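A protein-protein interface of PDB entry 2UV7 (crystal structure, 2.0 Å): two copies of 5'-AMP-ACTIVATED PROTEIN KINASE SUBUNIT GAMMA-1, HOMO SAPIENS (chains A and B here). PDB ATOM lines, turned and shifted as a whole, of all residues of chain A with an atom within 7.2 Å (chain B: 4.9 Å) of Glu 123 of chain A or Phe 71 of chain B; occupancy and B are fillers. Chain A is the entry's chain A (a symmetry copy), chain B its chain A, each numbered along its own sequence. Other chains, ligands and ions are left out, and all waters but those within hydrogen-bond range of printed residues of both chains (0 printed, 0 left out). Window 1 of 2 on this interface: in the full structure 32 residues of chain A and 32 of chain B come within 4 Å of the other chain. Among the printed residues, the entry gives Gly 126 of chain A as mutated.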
ATOM      1  N   HIS A  98      -5.274  13.034   2.710  1.00  0.00           N
ATOM      2  CA  HIS A  98      -6.070  12.076   1.971  1.00  0.00           C
ATOM      3  C   HIS A  98      -6.826  11.199   2.973  1.00  0.00           C
ATOM      4  O   HIS A  98      -7.988  10.892   2.783  1.00  0.00           O
ATOM      5  CB  HIS A  98      -5.164  11.214   1.077  1.00  0.00           C
ATOM      6  CG  HIS A  98      -4.419  11.994   0.032  1.00  0.00           C
ATOM      7  ND1 HIS A  98      -5.048  12.836  -0.866  1.00  0.00           N
ATOM      8  CD2 HIS A  98      -3.099  12.045  -0.267  1.00  0.00           C
ATOM      9  CE1 HIS A  98      -4.145  13.369  -1.672  1.00  0.00           C
ATOM     10  NE2 HIS A  98      -2.955  12.908  -1.329  1.00  0.00           N
ATOM     11  N   VAL A 103     -10.261   9.815   1.121  1.00  0.00           N
ATOM     12  CA  VAL A 103      -9.893   9.687  -0.297  1.00  0.00           C
ATOM     13  C   VAL A 103      -8.488   9.056  -0.428  1.00  0.00           C
ATOM     14  O   VAL A 103      -7.677   9.398  -1.317  1.00  0.00           O
ATOM     15  CB  VAL A 103     -10.001  11.075  -1.001  1.00  0.00           C
ATOM     16  CG1 VAL A 103     -11.470  11.521  -1.064  1.00  0.00           C
ATOM     17  CG2 VAL A 103      -9.147  12.144  -0.285  1.00  0.00           C
ATOM     18  N   ILE A 116     -14.792   5.653  -8.547  1.00  0.00           N
ATOM     19  CA  ILE A 116     -14.787   6.836  -9.425  1.00  0.00           C
ATOM     20  C   ILE A 116     -15.261   8.105  -8.698  1.00  0.00           C
ATOM     21  O   ILE A 116     -14.618   9.155  -8.798  1.00  0.00           O
ATOM     22  CB  ILE A 116     -15.616   6.596 -10.712  1.00  0.00           C
ATOM     23  CG1 ILE A 116     -14.885   5.618 -11.638  1.00  0.00           C
ATOM     24  CG2 ILE A 116     -15.837   7.890 -11.510  1.00  0.00           C
ATOM     25  CD1 ILE A 116     -15.700   5.251 -12.842  1.00  0.00           C
ATOM     26  N   ASN A 117     -16.361   8.007  -7.950  1.00  0.00           N
ATOM     27  CA  ASN A 117     -16.868   9.168  -7.174  1.00  0.00           C
ATOM     28  C   ASN A 117     -15.866   9.660  -6.120  1.00  0.00           C
ATOM     29  O   ASN A 117     -15.752  10.860  -5.894  1.00  0.00           O
ATOM     30  CB  ASN A 117     -18.234   8.880  -6.529  1.00  0.00           C
ATOM     31  CG  ASN A 117     -19.376   8.876  -7.540  1.00  0.00           C
ATOM     32  OD1 ASN A 117     -19.273   9.458  -8.613  1.00  0.00           O
ATOM     33  ND2 ASN A 117     -20.470   8.204  -7.197  1.00  0.00           N
ATOM     34  N   ARG A 118     -15.118   8.731  -5.531  1.00  0.00           N
ATOM     35  CA  ARG A 118     -14.095   9.034  -4.532  1.00  0.00           C
ATOM     36  C   ARG A 118     -12.890   9.742  -5.134  1.00  0.00           C
ATOM     37  O   ARG A 118     -12.428  10.742  -4.580  1.00  0.00           O
ATOM     38  CB  ARG A 118     -13.688   7.741  -3.768  1.00  0.00           C
ATOM     39  CG  ARG A 118     -12.671   7.949  -2.656  1.00  0.00           C
ATOM     40  CD  ARG A 118     -12.456   6.704  -1.772  1.00  0.00           C
ATOM     41  NE  ARG A 118     -13.722   6.237  -1.230  1.00  0.00           N
ATOM     42  CZ  ARG A 118     -14.069   4.966  -1.039  1.00  0.00           C
ATOM     43  NH1 ARG A 118     -13.230   3.961  -1.266  1.00  0.00           N
ATOM     44  NH2 ARG A 118     -15.281   4.708  -0.597  1.00  0.00           N
ATOM     45  N   LEU A 119     -12.419   9.272  -6.289  1.00  0.00           N
ATOM     46  CA  LEU A 119     -11.337   9.937  -7.036  1.00  0.00           C
ATOM     47  C   LEU A 119     -11.684  11.379  -7.351  1.00  0.00           C
ATOM     48  O   LEU A 119     -10.884  12.295  -7.105  1.00  0.00           O
ATOM     49  CB  LEU A 119     -10.990   9.176  -8.336  1.00  0.00           C
ATOM     50  CG  LEU A 119     -10.387   7.778  -8.151  1.00  0.00           C
ATOM     51  CD1 LEU A 119     -10.248   6.984  -9.478  1.00  0.00           C
ATOM     52  CD2 LEU A 119      -9.032   7.866  -7.420  1.00  0.00           C
ATOM     53  N   VAL A 120     -12.886  11.573  -7.881  1.00  0.00           N
ATOM     54  CA  VAL A 120     -13.379  12.877  -8.333  1.00  0.00           C
ATOM     55  C   VAL A 120     -13.629  13.858  -7.155  1.00  0.00           C
ATOM     56  O   VAL A 120     -13.351  15.045  -7.273  1.00  0.00           O
ATOM     57  CB  VAL A 120     -14.637  12.672  -9.255  1.00  0.00           C
ATOM     58  CG1 VAL A 120     -15.426  13.938  -9.458  1.00  0.00           C
ATOM     59  CG2 VAL A 120     -14.209  12.085 -10.616  1.00  0.00           C
ATOM     60  N   GLU A 121     -14.112  13.325  -6.033  1.00  0.00           N
ATOM     61  CA  GLU A 121     -14.322  14.038  -4.772  1.00  0.00           C
ATOM     62  C   GLU A 121     -13.176  14.970  -4.360  1.00  0.00           C
ATOM     63  O   GLU A 121     -13.417  16.136  -4.067  1.00  0.00           O
ATOM     64  CB  GLU A 121     -14.571  13.029  -3.632  1.00  0.00           C
ATOM     65  CG  GLU A 121     -15.408  13.560  -2.470  1.00  0.00           C
ATOM     66  CD  GLU A 121     -15.744  12.483  -1.428  1.00  0.00           C
ATOM     67  OE1 GLU A 121     -15.695  11.275  -1.747  1.00  0.00           O
ATOM     68  OE2 GLU A 121     -16.063  12.853  -0.278  1.00  0.00           O
ATOM     69  N   ALA A 122     -11.950  14.453  -4.340  1.00  0.00           N
ATOM     70  CA  ALA A 122     -10.754  15.246  -3.992  1.00  0.00           C
ATOM     71  C   ALA A 122      -9.798  15.456  -5.154  1.00  0.00           C
ATOM     72  O   ALA A 122      -8.697  15.949  -4.956  1.00  0.00           O
ATOM     73  CB  ALA A 122     -10.002  14.564  -2.859  1.00  0.00           C
ATOM     74  N   GLU A 123     -10.181  15.056  -6.363  1.00  0.00           N
ATOM     75  CA  GLU A 123      -9.272  15.147  -7.493  1.00  0.00           C
ATOM     76  C   GLU A 123      -7.944  14.453  -7.192  1.00  0.00           C
ATOM     77  O   GLU A 123      -6.872  15.059  -7.268  1.00  0.00           O
ATOM     78  CB  GLU A 123      -9.037  16.615  -7.883  1.00  0.00           C
ATOM     79  CG  GLU A 123     -10.337  17.374  -8.190  1.00  0.00           C
ATOM     80  CD  GLU A 123     -10.104  18.822  -8.610  1.00  0.00           C
ATOM     81  OE1 GLU A 123     -10.094  19.090  -9.838  1.00  0.00           O
ATOM     82  OE2 GLU A 123      -9.930  19.681  -7.711  1.00  0.00           O
ATOM     83  N   VAL A 124      -8.035  13.174  -6.851  1.00  0.00           N
ATOM     84  CA  VAL A 124      -6.857  12.346  -6.612  1.00  0.00           C
ATOM     85  C   VAL A 124      -6.734  11.291  -7.709  1.00  0.00           C
ATOM     86  O   VAL A 124      -7.735  10.889  -8.313  1.00  0.00           O
ATOM     87  CB  VAL A 124      -6.893  11.704  -5.181  1.00  0.00           C
ATOM     88  CG1 VAL A 124      -6.862  12.793  -4.127  1.00  0.00           C
ATOM     89  CG2 VAL A 124      -8.113  10.795  -4.987  1.00  0.00           C
ATOM     90  N   HIS A 125      -5.499  10.855  -7.960  1.00  0.00           N
ATOM     91  CA  HIS A 125      -5.202   9.963  -9.061  1.00  0.00           C
ATOM     92  C   HIS A 125      -5.058   8.490  -8.660  1.00  0.00           C
ATOM     93  O   HIS A 125      -4.855   7.620  -9.516  1.00  0.00           O
ATOM     94  CB  HIS A 125      -3.930  10.458  -9.757  1.00  0.00           C
ATOM     95  CG  HIS A 125      -4.136  11.728 -10.523  1.00  0.00           C
ATOM     96  ND1 HIS A 125      -3.611  11.931 -11.779  1.00  0.00           N
ATOM     97  CD2 HIS A 125      -4.850  12.840 -10.228  1.00  0.00           C
ATOM     98  CE1 HIS A 125      -3.985  13.122 -12.216  1.00  0.00           C
ATOM     99  NE2 HIS A 125      -4.731  13.695 -11.291  1.00  0.00           N
ATOM    100  N   GLY A 126      -5.207   8.199  -7.366  1.00  0.00           N
ATOM    101  CA  GLY A 126      -4.992   6.839  -6.892  1.00  0.00           C
ATOM    102  C   GLY A 126      -5.536   6.572  -5.502  1.00  0.00           C
ATOM    103  O   GLY A 126      -5.725   7.484  -4.699  1.00  0.00           O
ATOM    104  N   LEU A 142      -5.450   5.819 -12.050  1.00  0.00           N
ATOM    105  CA  LEU A 142      -6.311   6.220 -13.173  1.00  0.00           C
ATOM    106  C   LEU A 142      -6.172   5.277 -14.378  1.00  0.00           C
ATOM    107  O   LEU A 142      -7.173   4.953 -14.979  1.00  0.00           O
ATOM    108  CB  LEU A 142      -6.047   7.673 -13.577  1.00  0.00           C
ATOM    109  CG  LEU A 142      -6.281   8.739 -12.501  1.00  0.00           C
ATOM    110  CD1 LEU A 142      -6.081  10.122 -13.100  1.00  0.00           C
ATOM    111  CD2 LEU A 142      -7.674   8.600 -11.860  1.00  0.00           C
ATOM    112  N   LEU A 146      -9.233   3.312 -16.342  1.00  0.00           N
ATOM    113  CA  LEU A 146      -9.420   3.443 -17.802  1.00  0.00           C
ATOM    114  C   LEU A 146      -9.537   2.087 -18.504  1.00  0.00           C
ATOM    115  O   LEU A 146     -10.394   1.919 -19.369  1.00  0.00           O
ATOM    116  CB  LEU A 146      -8.310   4.322 -18.429  1.00  0.00           C
ATOM    117  CG  LEU A 146      -8.423   5.830 -18.148  1.00  0.00           C
ATOM    118  CD1 LEU A 146      -7.346   6.629 -18.870  1.00  0.00           C
ATOM    119  CD2 LEU A 146      -9.787   6.309 -18.548  1.00  0.00           C
ATOM    120  N   SER B  69      -6.383  14.995 -20.085  1.00  0.00           N
ATOM    121  CA  SER B  69      -5.716  14.047 -19.229  1.00  0.00           C
ATOM    122  C   SER B  69      -6.628  12.877 -18.888  1.00  0.00           C
ATOM    123  O   SER B  69      -7.830  12.892 -19.161  1.00  0.00           O
ATOM    124  CB  SER B  69      -5.256  14.748 -17.947  1.00  0.00           C
ATOM    125  OG  SER B  69      -6.360  15.038 -17.083  1.00  0.00           O
ATOM    126  N   LYS B  70      -6.030  11.859 -18.274  1.00  0.00           N
ATOM    127  CA  LYS B  70      -6.763  10.676 -17.837  1.00  0.00           C
ATOM    128  C   LYS B  70      -7.800  11.056 -16.806  1.00  0.00           C
ATOM    129  O   LYS B  70      -8.895  10.470 -16.792  1.00  0.00           O
ATOM    130  CB  LYS B  70      -5.801   9.633 -17.267  1.00  0.00           C
ATOM    131  CG  LYS B  70      -4.887   9.047 -18.302  1.00  0.00           C
ATOM    132  CD  LYS B  70      -3.855   8.133 -17.686  1.00  0.00           C
ATOM    133  CE  LYS B  70      -3.034   7.408 -18.746  1.00  0.00           C
ATOM    134  NZ  LYS B  70      -2.039   6.457 -18.166  1.00  0.00           N
ATOM    135  N   PHE B  71      -7.479  12.031 -15.947  1.00  0.00           N
ATOM    136  CA  PHE B  71      -8.458  12.513 -14.951  1.00  0.00           C
ATOM    137  C   PHE B  71      -9.727  13.112 -15.603  1.00  0.00           C
ATOM    138  O   PHE B  71     -10.855  12.963 -15.091  1.00  0.00           O
ATOM    139  CB  PHE B  71      -7.844  13.520 -13.947  1.00  0.00           C
ATOM    140  CG  PHE B  71      -8.799  13.880 -12.849  1.00  0.00           C
ATOM    141  CD1 PHE B  71      -9.060  12.974 -11.821  1.00  0.00           C
ATOM    142  CD2 PHE B  71      -9.532  15.061 -12.900  1.00  0.00           C
ATOM    143  CE1 PHE B  71      -9.988  13.273 -10.824  1.00  0.00           C
ATOM    144  CE2 PHE B  71     -10.461  15.366 -11.901  1.00  0.00           C
ATOM    145  CZ  PHE B  71     -10.697  14.470 -10.872  1.00  0.00           C
ATOM    146  N   ASP B  72      -9.543  13.775 -16.739  1.00  0.00           N
ATOM    147  CA  ASP B  72     -10.675  14.260 -17.527  1.00  0.00           C
ATOM    148  C   ASP B  72     -11.693  13.178 -17.881  1.00  0.00           C
ATOM    149  O   ASP B  72     -12.904  13.415 -17.796  1.00  0.00           O
ATOM    150  CB  ASP B  72     -10.178  14.995 -18.775  1.00  0.00           C
ATOM    151  CG  ASP B  72      -9.442  16.285 -18.412  1.00  0.00           C
ATOM    152  OD1 ASP B  72      -9.755  16.895 -17.356  1.00  0.00           O
ATOM    153  OD2 ASP B  72      -8.532  16.673 -19.142  1.00  0.00           O
ATOM    154  N   VAL B  73     -11.208  12.004 -18.285  1.00  0.00           N
ATOM    155  CA  VAL B  73     -12.082  10.865 -18.554  1.00  0.00           C
ATOM    156  C   VAL B  73     -12.857  10.414 -17.304  1.00  0.00           C
ATOM    157  O   VAL B  73     -14.054  10.108 -17.394  1.00  0.00           O
ATOM    158  CB  VAL B  73     -11.294   9.677 -19.152  1.00  0.00           C
ATOM    159  CG1 VAL B  73     -12.213   8.464 -19.417  1.00  0.00           C
ATOM    160  CG2 VAL B  73     -10.631  10.128 -20.405  1.00  0.00           C
ATOM    161  N   ILE B  74     -12.166  10.352 -16.161  1.00  0.00           N
ATOM    162  CA  ILE B  74     -12.780   9.963 -14.891  1.00  0.00           C
ATOM    163  C   ILE B  74     -13.837  10.996 -14.481  1.00  0.00           C
ATOM    164  O   ILE B  74     -14.926  10.643 -14.073  1.00  0.00           O
ATOM    165  CB  ILE B  74     -11.680   9.759 -13.774  1.00  0.00           C
ATOM    166  CG1 ILE B  74     -10.785   8.563 -14.116  1.00  0.00           C
ATOM    167  CG2 ILE B  74     -12.279   9.586 -12.383  1.00  0.00           C
ATOM    168  CD1 ILE B  74     -11.505   7.392 -14.700  1.00  0.00           C
ATOM    169  N   ASN B  75     -13.501  12.269 -14.613  1.00  0.00           N
ATOM    170  CA  ASN B  75     -14.454  13.361 -14.413  1.00  0.00           C
ATOM    171  C   ASN B  75     -15.731  13.205 -15.288  1.00  0.00           C
ATOM    172  O   ASN B  75     -16.837  13.261 -14.776  1.00  0.00           O
ATOM    173  CB  ASN B  75     -13.751  14.686 -14.686  1.00  0.00           C
ATOM    174  CG  ASN B  75     -13.996  15.726 -13.619  1.00  0.00           C
ATOM    175  OD1 ASN B  75     -14.765  15.525 -12.669  1.00  0.00           O
ATOM    176  ND2 ASN B  75     -13.335  16.870 -13.781  1.00  0.00           N
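N of Phe 71 of chain B sits close to OG of Ser 69 of chain B (3.4 Å).
O of Leu 119 of chain A sits at hydrogen-bond distance from N of Val 124 of chain A, at 3.0 Å.
The backbone NH (N) of Leu 142 of chain A is in hydrogen-bond range of the backbone carbonyl oxygen (O) of His 125 of chain A, at 3.2 Å.
O of Ile 74 of chain B touches CG2 of Ile 116 of chain A, 3.9 Å away.
O of Leu 119 of chain A touches CE1 of Phe 71 of chain B (3.9 Å).
CG2 of Val 120 of chain A touches CG2 of Ile 74 of chain B (3.6 Å).
Val 120 of chain A touches Asn 75 of chain B (CG1 to OD1, 3.6 Å).
Glu 123 of chain A touches Phe 71 of chain B.
Leu 142 of chain A touches Phe 71 of chain B (CD1 to N, 3.7 Å).
CG1 of Ile 74 of chain B touches CD2 of Leu 142 of chain A, at 3.8 Å.
Leu 146 of chain A touches Lys 70 of chain B (CD1 to CG, 3.5 Å).
Leu 146 of chain A touches Val 73 of chain B.
Of chain A, only Leu 119, Glu 123 and Leu 142 come within 4 Å of Phe 71 of chain B.
Printed residues of chain B within 4 Å of Ile 116 of chain A: Ile 74 (3.9 Å).
Of the printed residues of chain A, Val 73 of chain B touches Leu 146 (3.4 Å).
His 125 of chain A touches none of the printed residues of chain B.
Arg 118 of chain A touches none of the printed residues of chain B.
The nearest printed residue of chain B that does not touch Glu 123 of chain A is Asn 75 of chain B (5.6 Å).
The nearest residue of chain A that does not touch Phe 71 of chain B is Val 120 of chain A (4.02 Å).
The nearest printed residue of chain B that does not touch Leu 119 of chain A is Ile 74 of chain B (4.3 Å).
Of the 15 printed residues of chain A, 6 touch a printed residue of chain B.
Printed residues of chain A that touch a printed residue of chain B: Ile 116, Leu 119, Val 120, Glu 123, Leu 142 and Leu 146.
Along chain A the printed residues that touch a printed residue of chain B span positions 116 to 146.
Hydrophobic or aromatic side chains of chain B within 4 Å of the printed part of chain A: Phe 71, Val 73 and Ile 74.
Among the printed residues, no Asp or Glu carboxylate lies within 4 Å of a Lys or Arg side-chain nitrogen of the other chain.
No position is printed for both chains.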
